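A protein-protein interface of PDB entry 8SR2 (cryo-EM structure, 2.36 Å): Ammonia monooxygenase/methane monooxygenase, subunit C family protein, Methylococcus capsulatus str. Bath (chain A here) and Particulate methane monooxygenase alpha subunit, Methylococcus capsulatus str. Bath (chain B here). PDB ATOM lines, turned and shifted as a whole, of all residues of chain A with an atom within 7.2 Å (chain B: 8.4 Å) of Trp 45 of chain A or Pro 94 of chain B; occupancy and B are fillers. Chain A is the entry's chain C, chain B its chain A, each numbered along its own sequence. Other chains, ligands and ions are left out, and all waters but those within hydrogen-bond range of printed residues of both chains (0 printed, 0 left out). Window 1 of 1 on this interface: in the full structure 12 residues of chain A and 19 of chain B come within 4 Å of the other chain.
The backbone carbonyl oxygen (O) of Thr 133 of chain A sits close to the backbone carbonyl oxygen (O) of Met 93 of chain B (3.3 Å).
Printed residues of chain B that touch a printed residue of chain A: His 33, Met 93, Pro 94 and Gly 95. Along chain A the printed residues that touch a printed residue of chain B span positions 45 to 133.
The side-chain sulfur (SD) of Met 93 of chain B lies close to the backbone NH (N) of Phe 98 of chain B. N of Leu 49 of chain A sits at hydrogen-bond distance from O of Gly 44 of chain A (3.4 Å). The backbone carbonyl oxygen (O) of Trp 130 of chain A sits at hydrogen-bond distance from the side-chain hydroxyl (OG1) of Thr 133 of chain A (2.8 Å).
Among the printed residues, pairs that only touch across the chains: Trp 45 of chain A with Pro 94 of chain B (3.1 Å), Leu 49 of chain A with His 33 of chain B (3.3 Å), Leu 49 of chain A with Pro 94 of chain B (3.9 Å), Asp 50 of chain A with His 33 of chain B (3.97 Å) and Thr 133 of chain A with Gly 95 of chain B (3.8 Å).
Gly 41 of chain A touches none of the printed residues of chain B. Trp 45 of chain A touches one residue of chain B. Of the printed residues of chain B, Thr 133 of chain A touches Met 93 and Gly 95. Of the printed residues of chain A, His 33 of chain B touches Leu 49 and Asp 50. Printed residues of chain A within 4 Å of Met 93 of chain B: Thr 133. Of chain A, only Trp 45 and Leu 49 come within 4 Å of Pro 94 of chain B. The nearest residue of chain A that does not touch Pro 94 of chain B is Ile 134 of chain A (4.2 Å). The nearest printed residue of chain A that does not touch Gly 95 of chain B is Ile 134 of chain A (4.7 Å).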
ATOM      1  N   ARG A  37       4.326   7.709  13.781  1.00  0.00           N
ATOM      2  CA  ARG A  37       4.143   6.396  13.185  1.00  0.00           C
ATOM      3  C   ARG A  37       2.711   6.278  12.677  1.00  0.00           C
ATOM      4  O   ARG A  37       2.465   5.705  11.617  1.00  0.00           O
ATOM      5  CB  ARG A  37       4.438   5.299  14.209  1.00  0.00           C
ATOM      6  CG  ARG A  37       4.041   3.905  13.762  1.00  0.00           C
ATOM      7  CD  ARG A  37       4.981   3.375  12.694  1.00  0.00           C
ATOM      8  NE  ARG A  37       4.585   2.049  12.233  1.00  0.00           N
ATOM      9  CZ  ARG A  37       3.426   1.780  11.642  1.00  0.00           C
ATOM     10  NH1 ARG A  37       2.544   2.748  11.438  1.00  0.00           N
ATOM     11  NH2 ARG A  37       3.147   0.543  11.256  1.00  0.00           N
ATOM     12  N   GLU A  40       2.512   8.471   9.272  1.00  0.00           N
ATOM     13  CA  GLU A  40       3.105   7.724   8.170  1.00  0.00           C
ATOM     14  C   GLU A  40       2.400   6.389   7.946  1.00  0.00           C
ATOM     15  O   GLU A  40       2.416   5.848   6.843  1.00  0.00           O
ATOM     16  CB  GLU A  40       4.604   7.513   8.397  1.00  0.00           C
ATOM     17  CG  GLU A  40       4.942   6.458   9.433  1.00  0.00           C
ATOM     18  CD  GLU A  40       6.422   6.424   9.759  1.00  0.00           C
ATOM     19  OE1 GLU A  40       7.230   6.833   8.900  1.00  0.00           O
ATOM     20  OE2 GLU A  40       6.777   5.989  10.874  1.00  0.00           O
ATOM     21  N   GLY A  41       1.778   5.867   8.995  1.00  0.00           N
ATOM     22  CA  GLY A  41       1.068   4.606   8.898  1.00  0.00           C
ATOM     23  C   GLY A  41      -0.237   4.766   8.147  1.00  0.00           C
ATOM     24  O   GLY A  41      -0.720   3.834   7.505  1.00  0.00           O
ATOM     25  N   VAL A  42      -0.809   5.962   8.225  1.00  0.00           N
ATOM     26  CA  VAL A  42      -2.065   6.258   7.554  1.00  0.00           C
ATOM     27  C   VAL A  42      -1.822   6.923   6.204  1.00  0.00           C
ATOM     28  O   VAL A  42      -2.716   6.988   5.362  1.00  0.00           O
ATOM     29  CB  VAL A  42      -2.960   7.162   8.427  1.00  0.00           C
ATOM     30  CG1 VAL A  42      -3.682   8.195   7.577  1.00  0.00           C
ATOM     31  CG2 VAL A  42      -3.953   6.321   9.213  1.00  0.00           C
ATOM     32  N   TYR A  43      -0.601   7.406   5.994  1.00  0.00           N
ATOM     33  CA  TYR A  43      -0.265   8.073   4.739  1.00  0.00           C
ATOM     34  C   TYR A  43       0.914   7.457   3.986  1.00  0.00           C
ATOM     35  O   TYR A  43       1.666   8.170   3.326  1.00  0.00           O
ATOM     36  CB  TYR A  43      -0.029   9.568   4.973  1.00  0.00           C
ATOM     37  CG  TYR A  43      -1.257  10.303   5.455  1.00  0.00           C
ATOM     38  CD1 TYR A  43      -2.386  10.409   4.653  1.00  0.00           C
ATOM     39  CD2 TYR A  43      -1.294  10.889   6.713  1.00  0.00           C
ATOM     40  CE1 TYR A  43      -3.513  11.078   5.089  1.00  0.00           C
ATOM     41  CE2 TYR A  43      -2.417  11.559   7.158  1.00  0.00           C
ATOM     42  CZ  TYR A  43      -3.523  11.649   6.341  1.00  0.00           C
ATOM     43  OH  TYR A  43      -4.643  12.315   6.779  1.00  0.00           O
ATOM     44  N   GLY A  44       1.081   6.142   4.095  1.00  0.00           N
ATOM     45  CA  GLY A  44       2.138   5.446   3.379  1.00  0.00           C
ATOM     46  C   GLY A  44       1.617   5.325   1.963  1.00  0.00           C
ATOM     47  O   GLY A  44       1.951   6.128   1.097  1.00  0.00           O
ATOM     48  N   TRP A  45       0.796   4.301   1.748  1.00  0.00           N
ATOM     49  CA  TRP A  45       0.156   4.082   0.463  1.00  0.00           C
ATOM     50  C   TRP A  45      -0.958   5.118   0.383  1.00  0.00           C
ATOM     51  O   TRP A  45      -1.554   5.445   1.418  1.00  0.00           O
ATOM     52  CB  TRP A  45      -0.409   2.666   0.384  1.00  0.00           C
ATOM     53  CG  TRP A  45       0.370   1.678   1.195  1.00  0.00           C
ATOM     54  CD1 TRP A  45       1.129   0.647   0.724  1.00  0.00           C
ATOM     55  CD2 TRP A  45       0.473   1.633   2.622  1.00  0.00           C
ATOM     56  NE1 TRP A  45       1.695  -0.040   1.770  1.00  0.00           N
ATOM     57  CE2 TRP A  45       1.308   0.546   2.945  1.00  0.00           C
ATOM     58  CE3 TRP A  45      -0.060   2.405   3.659  1.00  0.00           C
ATOM     59  CZ2 TRP A  45       1.621   0.211   4.260  1.00  0.00           C
ATOM     60  CZ3 TRP A  45       0.251   2.071   4.962  1.00  0.00           C
ATOM     61  CH2 TRP A  45       1.085   0.984   5.252  1.00  0.00           C
ATOM     62  N   SER A  46      -1.211   5.598  -0.843  1.00  0.00           N
ATOM     63  CA  SER A  46      -2.186   6.648  -1.219  1.00  0.00           C
ATOM     64  C   SER A  46      -1.719   8.035  -0.762  1.00  0.00           C
ATOM     65  O   SER A  46      -1.606   8.308   0.433  1.00  0.00           O
ATOM     66  CB  SER A  46      -3.645   6.352  -0.821  1.00  0.00           C
ATOM     67  OG  SER A  46      -3.847   6.594   0.561  1.00  0.00           O
ATOM     68  N   ALA A  47      -1.443   8.895  -1.742  1.00  0.00           N
ATOM     69  CA  ALA A  47      -0.930  10.245  -1.505  1.00  0.00           C
ATOM     70  C   ALA A  47       0.285  10.163  -0.586  1.00  0.00           C
ATOM     71  O   ALA A  47       0.343  10.810   0.458  1.00  0.00           O
ATOM     72  CB  ALA A  47      -2.003  11.177  -0.946  1.00  0.00           C
ATOM     73  N   GLY A  48       1.245   9.341  -0.999  1.00  0.00           N
ATOM     74  CA  GLY A  48       2.475   9.116  -0.265  1.00  0.00           C
ATOM     75  C   GLY A  48       3.378   8.184  -1.053  1.00  0.00           C
ATOM     76  O   GLY A  48       4.591   8.158  -0.856  1.00  0.00           O
ATOM     77  N   LEU A  49       2.772   7.414  -1.953  1.00  0.00           N
ATOM     78  CA  LEU A  49       3.508   6.481  -2.796  1.00  0.00           C
ATOM     79  C   LEU A  49       4.072   7.217  -4.005  1.00  0.00           C
ATOM     80  O   LEU A  49       5.284   7.247  -4.211  1.00  0.00           O
ATOM     81  CB  LEU A  49       2.604   5.337  -3.249  1.00  0.00           C
ATOM     82  CG  LEU A  49       3.058   3.931  -2.855  1.00  0.00           C
ATOM     83  CD1 LEU A  49       4.194   4.000  -1.847  1.00  0.00           C
ATOM     84  CD2 LEU A  49       1.892   3.128  -2.301  1.00  0.00           C
ATOM     85  N   ASP A  50       3.189   7.803  -4.807  1.00  0.00           N
ATOM     86  CA  ASP A  50       3.623   8.559  -5.973  1.00  0.00           C
ATOM     87  C   ASP A  50       4.160   9.904  -5.510  1.00  0.00           C
ATOM     88  O   ASP A  50       3.440  10.680  -4.889  1.00  0.00           O
ATOM     89  CB  ASP A  50       2.458   8.760  -6.942  1.00  0.00           C
ATOM     90  CG  ASP A  50       2.872   9.479  -8.208  1.00  0.00           C
ATOM     91  OD1 ASP A  50       4.084   9.717  -8.388  1.00  0.00           O
ATOM     92  OD2 ASP A  50       1.986   9.808  -9.025  1.00  0.00           O
ATOM     93  N   TRP A  60       3.078  14.991   2.325  1.00  0.00           N
ATOM     94  CA  TRP A  60       4.465  14.670   2.643  1.00  0.00           C
ATOM     95  C   TRP A  60       5.428  15.817   2.367  1.00  0.00           C
ATOM     96  O   TRP A  60       6.424  15.976   3.068  1.00  0.00           O
ATOM     97  CB  TRP A  60       4.896  13.389   1.929  1.00  0.00           C
ATOM     98  CG  TRP A  60       4.236  12.183   2.511  1.00  0.00           C
ATOM     99  CD1 TRP A  60       3.299  11.393   1.916  1.00  0.00           C
ATOM    100  CD2 TRP A  60       4.444  11.642   3.819  1.00  0.00           C
ATOM    101  NE1 TRP A  60       2.918  10.386   2.767  1.00  0.00           N
ATOM    102  CE2 TRP A  60       3.607  10.517   3.944  1.00  0.00           C
ATOM    103  CE3 TRP A  60       5.263  11.996   4.895  1.00  0.00           C
ATOM    104  CZ2 TRP A  60       3.565   9.745   5.100  1.00  0.00           C
ATOM    105  CZ3 TRP A  60       5.218  11.228   6.041  1.00  0.00           C
ATOM    106  CH2 TRP A  60       4.376  10.114   6.135  1.00  0.00           C
ATOM    107  N   TRP A 130      10.244   0.098   4.563  1.00  0.00           N
ATOM    108  CA  TRP A 130       9.607   0.827   3.432  1.00  0.00           C
ATOM    109  C   TRP A 130      10.299   0.481   2.107  1.00  0.00           C
ATOM    110  O   TRP A 130       9.599   0.033   1.179  1.00  0.00           O
ATOM    111  CB  TRP A 130       9.600   2.338   3.694  1.00  0.00           C
ATOM    112  CG  TRP A 130       8.329   3.017   3.281  1.00  0.00           C
ATOM    113  CD1 TRP A 130       8.211   4.248   2.705  1.00  0.00           C
ATOM    114  CD2 TRP A 130       6.989   2.505   3.412  1.00  0.00           C
ATOM    115  NE1 TRP A 130       6.895   4.540   2.468  1.00  0.00           N
ATOM    116  CE2 TRP A 130       6.122   3.489   2.891  1.00  0.00           C
ATOM    117  CE3 TRP A 130       6.434   1.324   3.917  1.00  0.00           C
ATOM    118  CZ2 TRP A 130       4.737   3.324   2.861  1.00  0.00           C
ATOM    119  CZ3 TRP A 130       5.067   1.160   3.888  1.00  0.00           C
ATOM    120  CH2 TRP A 130       4.232   2.150   3.367  1.00  0.00           C
ATOM    121  N   THR A 133       9.962  -2.582   0.467  1.00  0.00           N
ATOM    122  CA  THR A 133       8.634  -2.829  -0.094  1.00  0.00           C
ATOM    123  C   THR A 133       8.317  -1.949  -1.299  1.00  0.00           C
ATOM    124  O   THR A 133       7.578  -2.383  -2.190  1.00  0.00           O
ATOM    125  CB  THR A 133       7.540  -2.662   0.967  1.00  0.00           C
ATOM    126  OG1 THR A 133       7.116  -1.293   1.022  1.00  0.00           O
ATOM    127  CG2 THR A 133       8.002  -3.142   2.324  1.00  0.00           C
ATOM    128  N   ILE A 134       8.830  -0.719  -1.355  1.00  0.00           N
ATOM    129  CA  ILE A 134       8.484   0.184  -2.445  1.00  0.00           C
ATOM    130  C   ILE A 134       9.749   0.743  -3.084  1.00  0.00           C
ATOM    131  O   ILE A 134      10.812   0.810  -2.469  1.00  0.00           O
ATOM    132  CB  ILE A 134       7.515   1.316  -1.984  1.00  0.00           C
ATOM    133  CG1 ILE A 134       8.162   2.368  -1.057  1.00  0.00           C
ATOM    134  CG2 ILE A 134       6.264   0.733  -1.337  1.00  0.00           C
ATOM    135  CD1 ILE A 134       9.063   3.418  -1.696  1.00  0.00           C
ATOM    136  N   PRO A 142       8.233   9.458   2.267  1.00  0.00           N
ATOM    137  CA  PRO A 142       7.550   9.473   3.562  1.00  0.00           C
ATOM    138  C   PRO A 142       8.480   9.137   4.708  1.00  0.00           C
ATOM    139  O   PRO A 142       8.552   9.874   5.690  1.00  0.00           O
ATOM    140  CB  PRO A 142       6.496   8.382   3.402  1.00  0.00           C
ATOM    141  CG  PRO A 142       6.164   8.415   1.952  1.00  0.00           C
ATOM    142  CD  PRO A 142       7.433   8.783   1.231  1.00  0.00           C
ATOM    143  N   HIS B  33       4.698   2.897  -9.471  1.00  0.00           N
ATOM    144  CA  HIS B  33       4.461   4.106  -8.689  1.00  0.00           C
ATOM    145  C   HIS B  33       5.869   4.663  -8.788  1.00  0.00           C
ATOM    146  O   HIS B  33       6.018   5.739  -9.336  1.00  0.00           O
ATOM    147  CB  HIS B  33       3.867   3.882  -7.256  1.00  0.00           C
ATOM    148  CG  HIS B  33       2.355   4.018  -7.182  1.00  0.00           C
ATOM    149  ND1 HIS B  33       1.554   3.643  -8.238  1.00  0.00           N
ATOM    150  CD2 HIS B  33       1.529   4.477  -6.215  1.00  0.00           C
ATOM    151  CE1 HIS B  33       0.292   3.867  -7.921  1.00  0.00           C
ATOM    152  NE2 HIS B  33       0.249   4.371  -6.700  1.00  0.00           N
ATOM    153  N   VAL B  91       7.494  -8.041  -9.329  1.00  0.00           N
ATOM    154  CA  VAL B  91       6.174  -7.429  -9.436  1.00  0.00           C
ATOM    155  C   VAL B  91       6.167  -6.169  -8.584  1.00  0.00           C
ATOM    156  O   VAL B  91       6.580  -6.199  -7.419  1.00  0.00           O
ATOM    157  CB  VAL B  91       5.056  -8.391  -8.988  1.00  0.00           C
ATOM    158  CG1 VAL B  91       3.703  -7.724  -9.126  1.00  0.00           C
ATOM    159  CG2 VAL B  91       5.104  -9.677  -9.797  1.00  0.00           C
ATOM    160  N   GLY B  92       5.700  -5.064  -9.163  1.00  0.00           N
ATOM    161  CA  GLY B  92       5.632  -3.808  -8.445  1.00  0.00           C
ATOM    162  C   GLY B  92       4.327  -3.609  -7.704  1.00  0.00           C
ATOM    163  O   GLY B  92       3.277  -3.413  -8.323  1.00  0.00           O
ATOM    164  N   MET B  93       4.378  -3.660  -6.375  1.00  0.00           N
ATOM    165  CA  MET B  93       3.192  -3.492  -5.546  1.00  0.00           C
ATOM    166  C   MET B  93       3.630  -2.981  -4.182  1.00  0.00           C
ATOM    167  O   MET B  93       4.774  -3.208  -3.771  1.00  0.00           O
ATOM    168  CB  MET B  93       2.419  -4.810  -5.408  1.00  0.00           C
ATOM    169  CG  MET B  93       3.225  -5.941  -4.796  1.00  0.00           C
ATOM    170  SD  MET B  93       2.299  -7.485  -4.740  1.00  0.00           S
ATOM    171  CE  MET B  93       1.508  -7.450  -6.344  1.00  0.00           C
ATOM    172  N   PRO B  94       2.723  -2.294  -3.472  1.00  0.00           N
ATOM    173  CA  PRO B  94       2.990  -1.731  -2.143  1.00  0.00           C
ATOM    174  C   PRO B  94       2.997  -2.802  -1.061  1.00  0.00           C
ATOM    175  O   PRO B  94       1.970  -3.034  -0.428  1.00  0.00           O
ATOM    176  CB  PRO B  94       1.808  -0.776  -1.915  1.00  0.00           C
ATOM    177  CG  PRO B  94       1.023  -0.760  -3.188  1.00  0.00           C
ATOM    178  CD  PRO B  94       1.347  -2.029  -3.908  1.00  0.00           C
ATOM    179  N   GLY B  95       4.142  -3.441  -0.851  1.00  0.00           N
ATOM    180  CA  GLY B  95       4.250  -4.489   0.147  1.00  0.00           C
ATOM    181  C   GLY B  95       3.684  -5.783  -0.396  1.00  0.00           C
ATOM    182  O   GLY B  95       3.525  -5.931  -1.597  1.00  0.00           O
ATOM    183  N   PRO B  96       3.444  -6.758   0.490  1.00  0.00           N
ATOM    184  CA  PRO B  96       2.913  -8.060   0.083  1.00  0.00           C
ATOM    185  C   PRO B  96       1.391  -8.093   0.041  1.00  0.00           C
ATOM    186  O   PRO B  96       0.775  -8.843   0.795  1.00  0.00           O
ATOM    187  CB  PRO B  96       3.429  -9.014   1.173  1.00  0.00           C
ATOM    188  CG  PRO B  96       4.253  -8.182   2.110  1.00  0.00           C
ATOM    189  CD  PRO B  96       3.847  -6.757   1.900  1.00  0.00           C
ATOM    190  N   VAL B  97       0.795  -7.293  -0.836  1.00  0.00           N
ATOM    191  CA  VAL B  97      -0.657  -7.268  -0.984  1.00  0.00           C
ATOM    192  C   VAL B  97      -1.096  -8.433  -1.869  1.00  0.00           C
ATOM    193  O   VAL B  97      -2.240  -8.877  -1.816  1.00  0.00           O
ATOM    194  CB  VAL B  97      -1.154  -5.937  -1.579  1.00  0.00           C
ATOM    195  CG1 VAL B  97      -0.842  -4.788  -0.635  1.00  0.00           C
ATOM    196  CG2 VAL B  97      -0.530  -5.695  -2.943  1.00  0.00           C
ATOM    197  N   PHE B  98      -0.164  -8.911  -2.685  1.00  0.00           N
ATOM    198  CA  PHE B  98      -0.380 -10.035  -3.577  1.00  0.00           C
ATOM    199  C   PHE B  98       0.838 -10.931  -3.439  1.00  0.00           C
ATOM    200  O   PHE B  98       1.968 -10.452  -3.487  1.00  0.00           O
ATOM    201  CB  PHE B  98      -0.465  -9.559  -5.025  1.00  0.00           C
ATOM    202  CG  PHE B  98      -1.808  -9.020  -5.415  1.00  0.00           C
ATOM    203  CD1 PHE B  98      -2.842  -9.875  -5.753  1.00  0.00           C
ATOM    204  CD2 PHE B  98      -2.030  -7.655  -5.462  1.00  0.00           C
ATOM    205  CE1 PHE B  98      -4.075  -9.379  -6.122  1.00  0.00           C
ATOM    206  CE2 PHE B  98      -3.261  -7.152  -5.830  1.00  0.00           C
ATOM    207  CZ  PHE B  98      -4.285  -8.016  -6.161  1.00  0.00           C
ATOM    208  N   ARG B 131      -4.056 -11.044  -1.106  1.00  0.00           N
ATOM    209  CA  ARG B 131      -3.765 -11.212   0.313  1.00  0.00           C
ATOM    210  C   ARG B 131      -4.291 -10.075   1.176  1.00  0.00           C
ATOM    211  O   ARG B 131      -4.755 -10.325   2.292  1.00  0.00           O
ATOM    212  CB  ARG B 131      -2.246 -11.358   0.514  1.00  0.00           C
ATOM    213  CG  ARG B 131      -1.822 -11.677   1.938  1.00  0.00           C
ATOM    214  CD  ARG B 131      -0.318 -11.889   2.021  1.00  0.00           C
ATOM    215  NE  ARG B 131       0.154 -11.982   3.397  1.00  0.00           N
ATOM    216  CZ  ARG B 131       0.794 -11.012   4.035  1.00  0.00           C
ATOM    217  NH1 ARG B 131       1.047  -9.851   3.454  1.00  0.00           N
ATOM    218  NH2 ARG B 131       1.193 -11.212   5.288  1.00  0.00           N
ATOM    219  N   ARG B 132      -4.242  -8.835   0.689  1.00  0.00           N
ATOM    220  CA  ARG B 132      -4.628  -7.676   1.480  1.00  0.00           C
ATOM    221  C   ARG B 132      -5.701  -6.887   0.740  1.00  0.00           C
ATOM    222  O   ARG B 132      -5.505  -6.524  -0.433  1.00  0.00           O
ATOM    223  CB  ARG B 132      -3.413  -6.785   1.770  1.00  0.00           C
ATOM    224  CG  ARG B 132      -2.805  -6.996   3.146  1.00  0.00           C
ATOM    225  CD  ARG B 132      -1.712  -5.979   3.427  1.00  0.00           C
ATOM    226  NE  ARG B 132      -2.258  -4.673   3.771  1.00  0.00           N
ATOM    227  CZ  ARG B 132      -1.667  -3.517   3.498  1.00  0.00           C
ATOM    228  NH1 ARG B 132      -0.503  -3.467   2.872  1.00  0.00           N
ATOM    229  NH2 ARG B 132      -2.259  -2.385   3.863  1.00  0.00           N
ATOM    230  N   ASP B 135      -7.140  -1.091  -2.910  1.00  0.00           N
ATOM    231  CA  ASP B 135      -6.852  -0.812  -4.314  1.00  0.00           C
ATOM    232  C   ASP B 135      -5.349  -0.679  -4.496  1.00  0.00           C
ATOM    233  O   ASP B 135      -4.729   0.219  -3.930  1.00  0.00           O
ATOM    234  CB  ASP B 135      -7.551   0.469  -4.760  1.00  0.00           C
ATOM    235  CG  ASP B 135      -8.957   0.220  -5.257  1.00  0.00           C
ATOM    236  OD1 ASP B 135      -9.109  -0.436  -6.307  1.00  0.00           O
ATOM    237  OD2 ASP B 135      -9.913   0.677  -4.594  1.00  0.00           O
ATOM    238  N   TRP B 136      -4.765  -1.569  -5.288  1.00  0.00           N
ATOM    239  CA  TRP B 136      -3.323  -1.553  -5.502  1.00  0.00           C
ATOM    240  C   TRP B 136      -2.908  -1.373  -6.956  1.00  0.00           C
ATOM    241  O   TRP B 136      -3.591  -1.822  -7.873  1.00  0.00           O
ATOM    242  CB  TRP B 136      -2.705  -2.832  -4.943  1.00  0.00           C
ATOM    243  CG  TRP B 136      -3.294  -3.247  -3.635  1.00  0.00           C
ATOM    244  CD1 TRP B 136      -4.124  -4.303  -3.409  1.00  0.00           C
ATOM    245  CD2 TRP B 136      -3.104  -2.606  -2.369  1.00  0.00           C
ATOM    246  NE1 TRP B 136      -4.461  -4.363  -2.080  1.00  0.00           N
ATOM    247  CE2 TRP B 136      -3.847  -3.332  -1.420  1.00  0.00           C
ATOM    248  CE3 TRP B 136      -2.376  -1.491  -1.948  1.00  0.00           C
ATOM    249  CZ2 TRP B 136      -3.882  -2.979  -0.075  1.00  0.00           C
ATOM    250  CZ3 TRP B 136      -2.412  -1.142  -0.614  1.00  0.00           C
ATOM    251  CH2 TRP B 136      -3.161  -1.882   0.307  1.00  0.00           C
ATOM    252  N   HIS B 137      -1.773  -0.710  -7.152  1.00  0.00           N
ATOM    253  CA  HIS B 137      -1.231  -0.475  -8.479  1.00  0.00           C
ATOM    254  C   HIS B 137      -0.162  -1.520  -8.761  1.00  0.00           C
ATOM    255  O   HIS B 137       0.969  -1.402  -8.291  1.00  0.00           O
ATOM    256  CB  HIS B 137      -0.631   0.927  -8.569  1.00  0.00           C
ATOM    257  CG  HIS B 137      -0.763   1.552  -9.921  1.00  0.00           C
ATOM    258  ND1 HIS B 137       0.219   2.344 -10.478  1.00  0.00           N
ATOM    259  CD2 HIS B 137      -1.766   1.503 -10.829  1.00  0.00           C
ATOM    260  CE1 HIS B 137      -0.174   2.753 -11.671  1.00  0.00           C
ATOM    261  NE2 HIS B 137      -1.375   2.257 -11.906  1.00  0.00           N
ATOM    262  N   VAL B 138      -0.522  -2.543  -9.526  1.00  0.00           N
ATOM    263  CA  VAL B 138       0.409  -3.618  -9.847  1.00  0.00           C
ATOM    264  C   VAL B 138       1.186  -3.376 -11.137  1.00  0.00           C
ATOM    265  O   VAL B 138       0.601  -3.137 -12.190  1.00  0.00           O
ATOM    266  CB  VAL B 138      -0.319  -4.970  -9.950  1.00  0.00           C
ATOM    267  CG1 VAL B 138       0.685  -6.110  -9.995  1.00  0.00           C
ATOM    268  CG2 VAL B 138      -1.279  -5.142  -8.785  1.00  0.00           C
ATOM    269  N   HIS B 139       2.512  -3.435 -11.040  1.00  0.00           N
ATOM    270  CA  HIS B 139       3.382  -3.241 -12.191  1.00  0.00           C
ATOM    271  C   HIS B 139       4.160  -4.518 -12.470  1.00  0.00           C
ATOM    272  O   HIS B 139       4.560  -5.222 -11.547  1.00  0.00           O
ATOM    273  CB  HIS B 139       4.399  -2.127 -11.933  1.00  0.00           C
ATOM    274  CG  HIS B 139       3.794  -0.771 -11.759  1.00  0.00           C
ATOM    275  ND1 HIS B 139       3.864   0.207 -12.729  1.00  0.00           N
ATOM    276  CD2 HIS B 139       3.135  -0.221 -10.714  1.00  0.00           C
ATOM    277  CE1 HIS B 139       3.258   1.297 -12.294  1.00  0.00           C
ATOM    278  NE2 HIS B 139       2.811   1.065 -11.074  1.00  0.00           N
ATOM    279  N   TRP B 156      -4.585  -0.791 -11.894  1.00  0.00           N
ATOM    280  CA  TRP B 156      -5.250  -0.807 -10.598  1.00  0.00           C
ATOM    281  C   TRP B 156      -6.078  -2.078 -10.455  1.00  0.00           C
ATOM    282  O   TRP B 156      -6.926  -2.376 -11.302  1.00  0.00           O
ATOM    283  CB  TRP B 156      -6.135   0.427 -10.445  1.00  0.00           C
ATOM    284  CG  TRP B 156      -5.370   1.694 -10.231  1.00  0.00           C
ATOM    285  CD1 TRP B 156      -5.111   2.661 -11.158  1.00  0.00           C
ATOM    286  CD2 TRP B 156      -4.766   2.138  -9.011  1.00  0.00           C
ATOM    287  NE1 TRP B 156      -4.381   3.677 -10.592  1.00  0.00           N
ATOM    288  CE2 TRP B 156      -4.157   3.380  -9.274  1.00  0.00           C
ATOM    289  CE3 TRP B 156      -4.681   1.603  -7.721  1.00  0.00           C
ATOM    290  CZ2 TRP B 156      -3.471   4.096  -8.296  1.00  0.00           C
ATOM    291  CZ3 TRP B 156      -4.001   2.317  -6.753  1.00  0.00           C
ATOM    292  CH2 TRP B 156      -3.404   3.549  -7.044  1.00  0.00           C
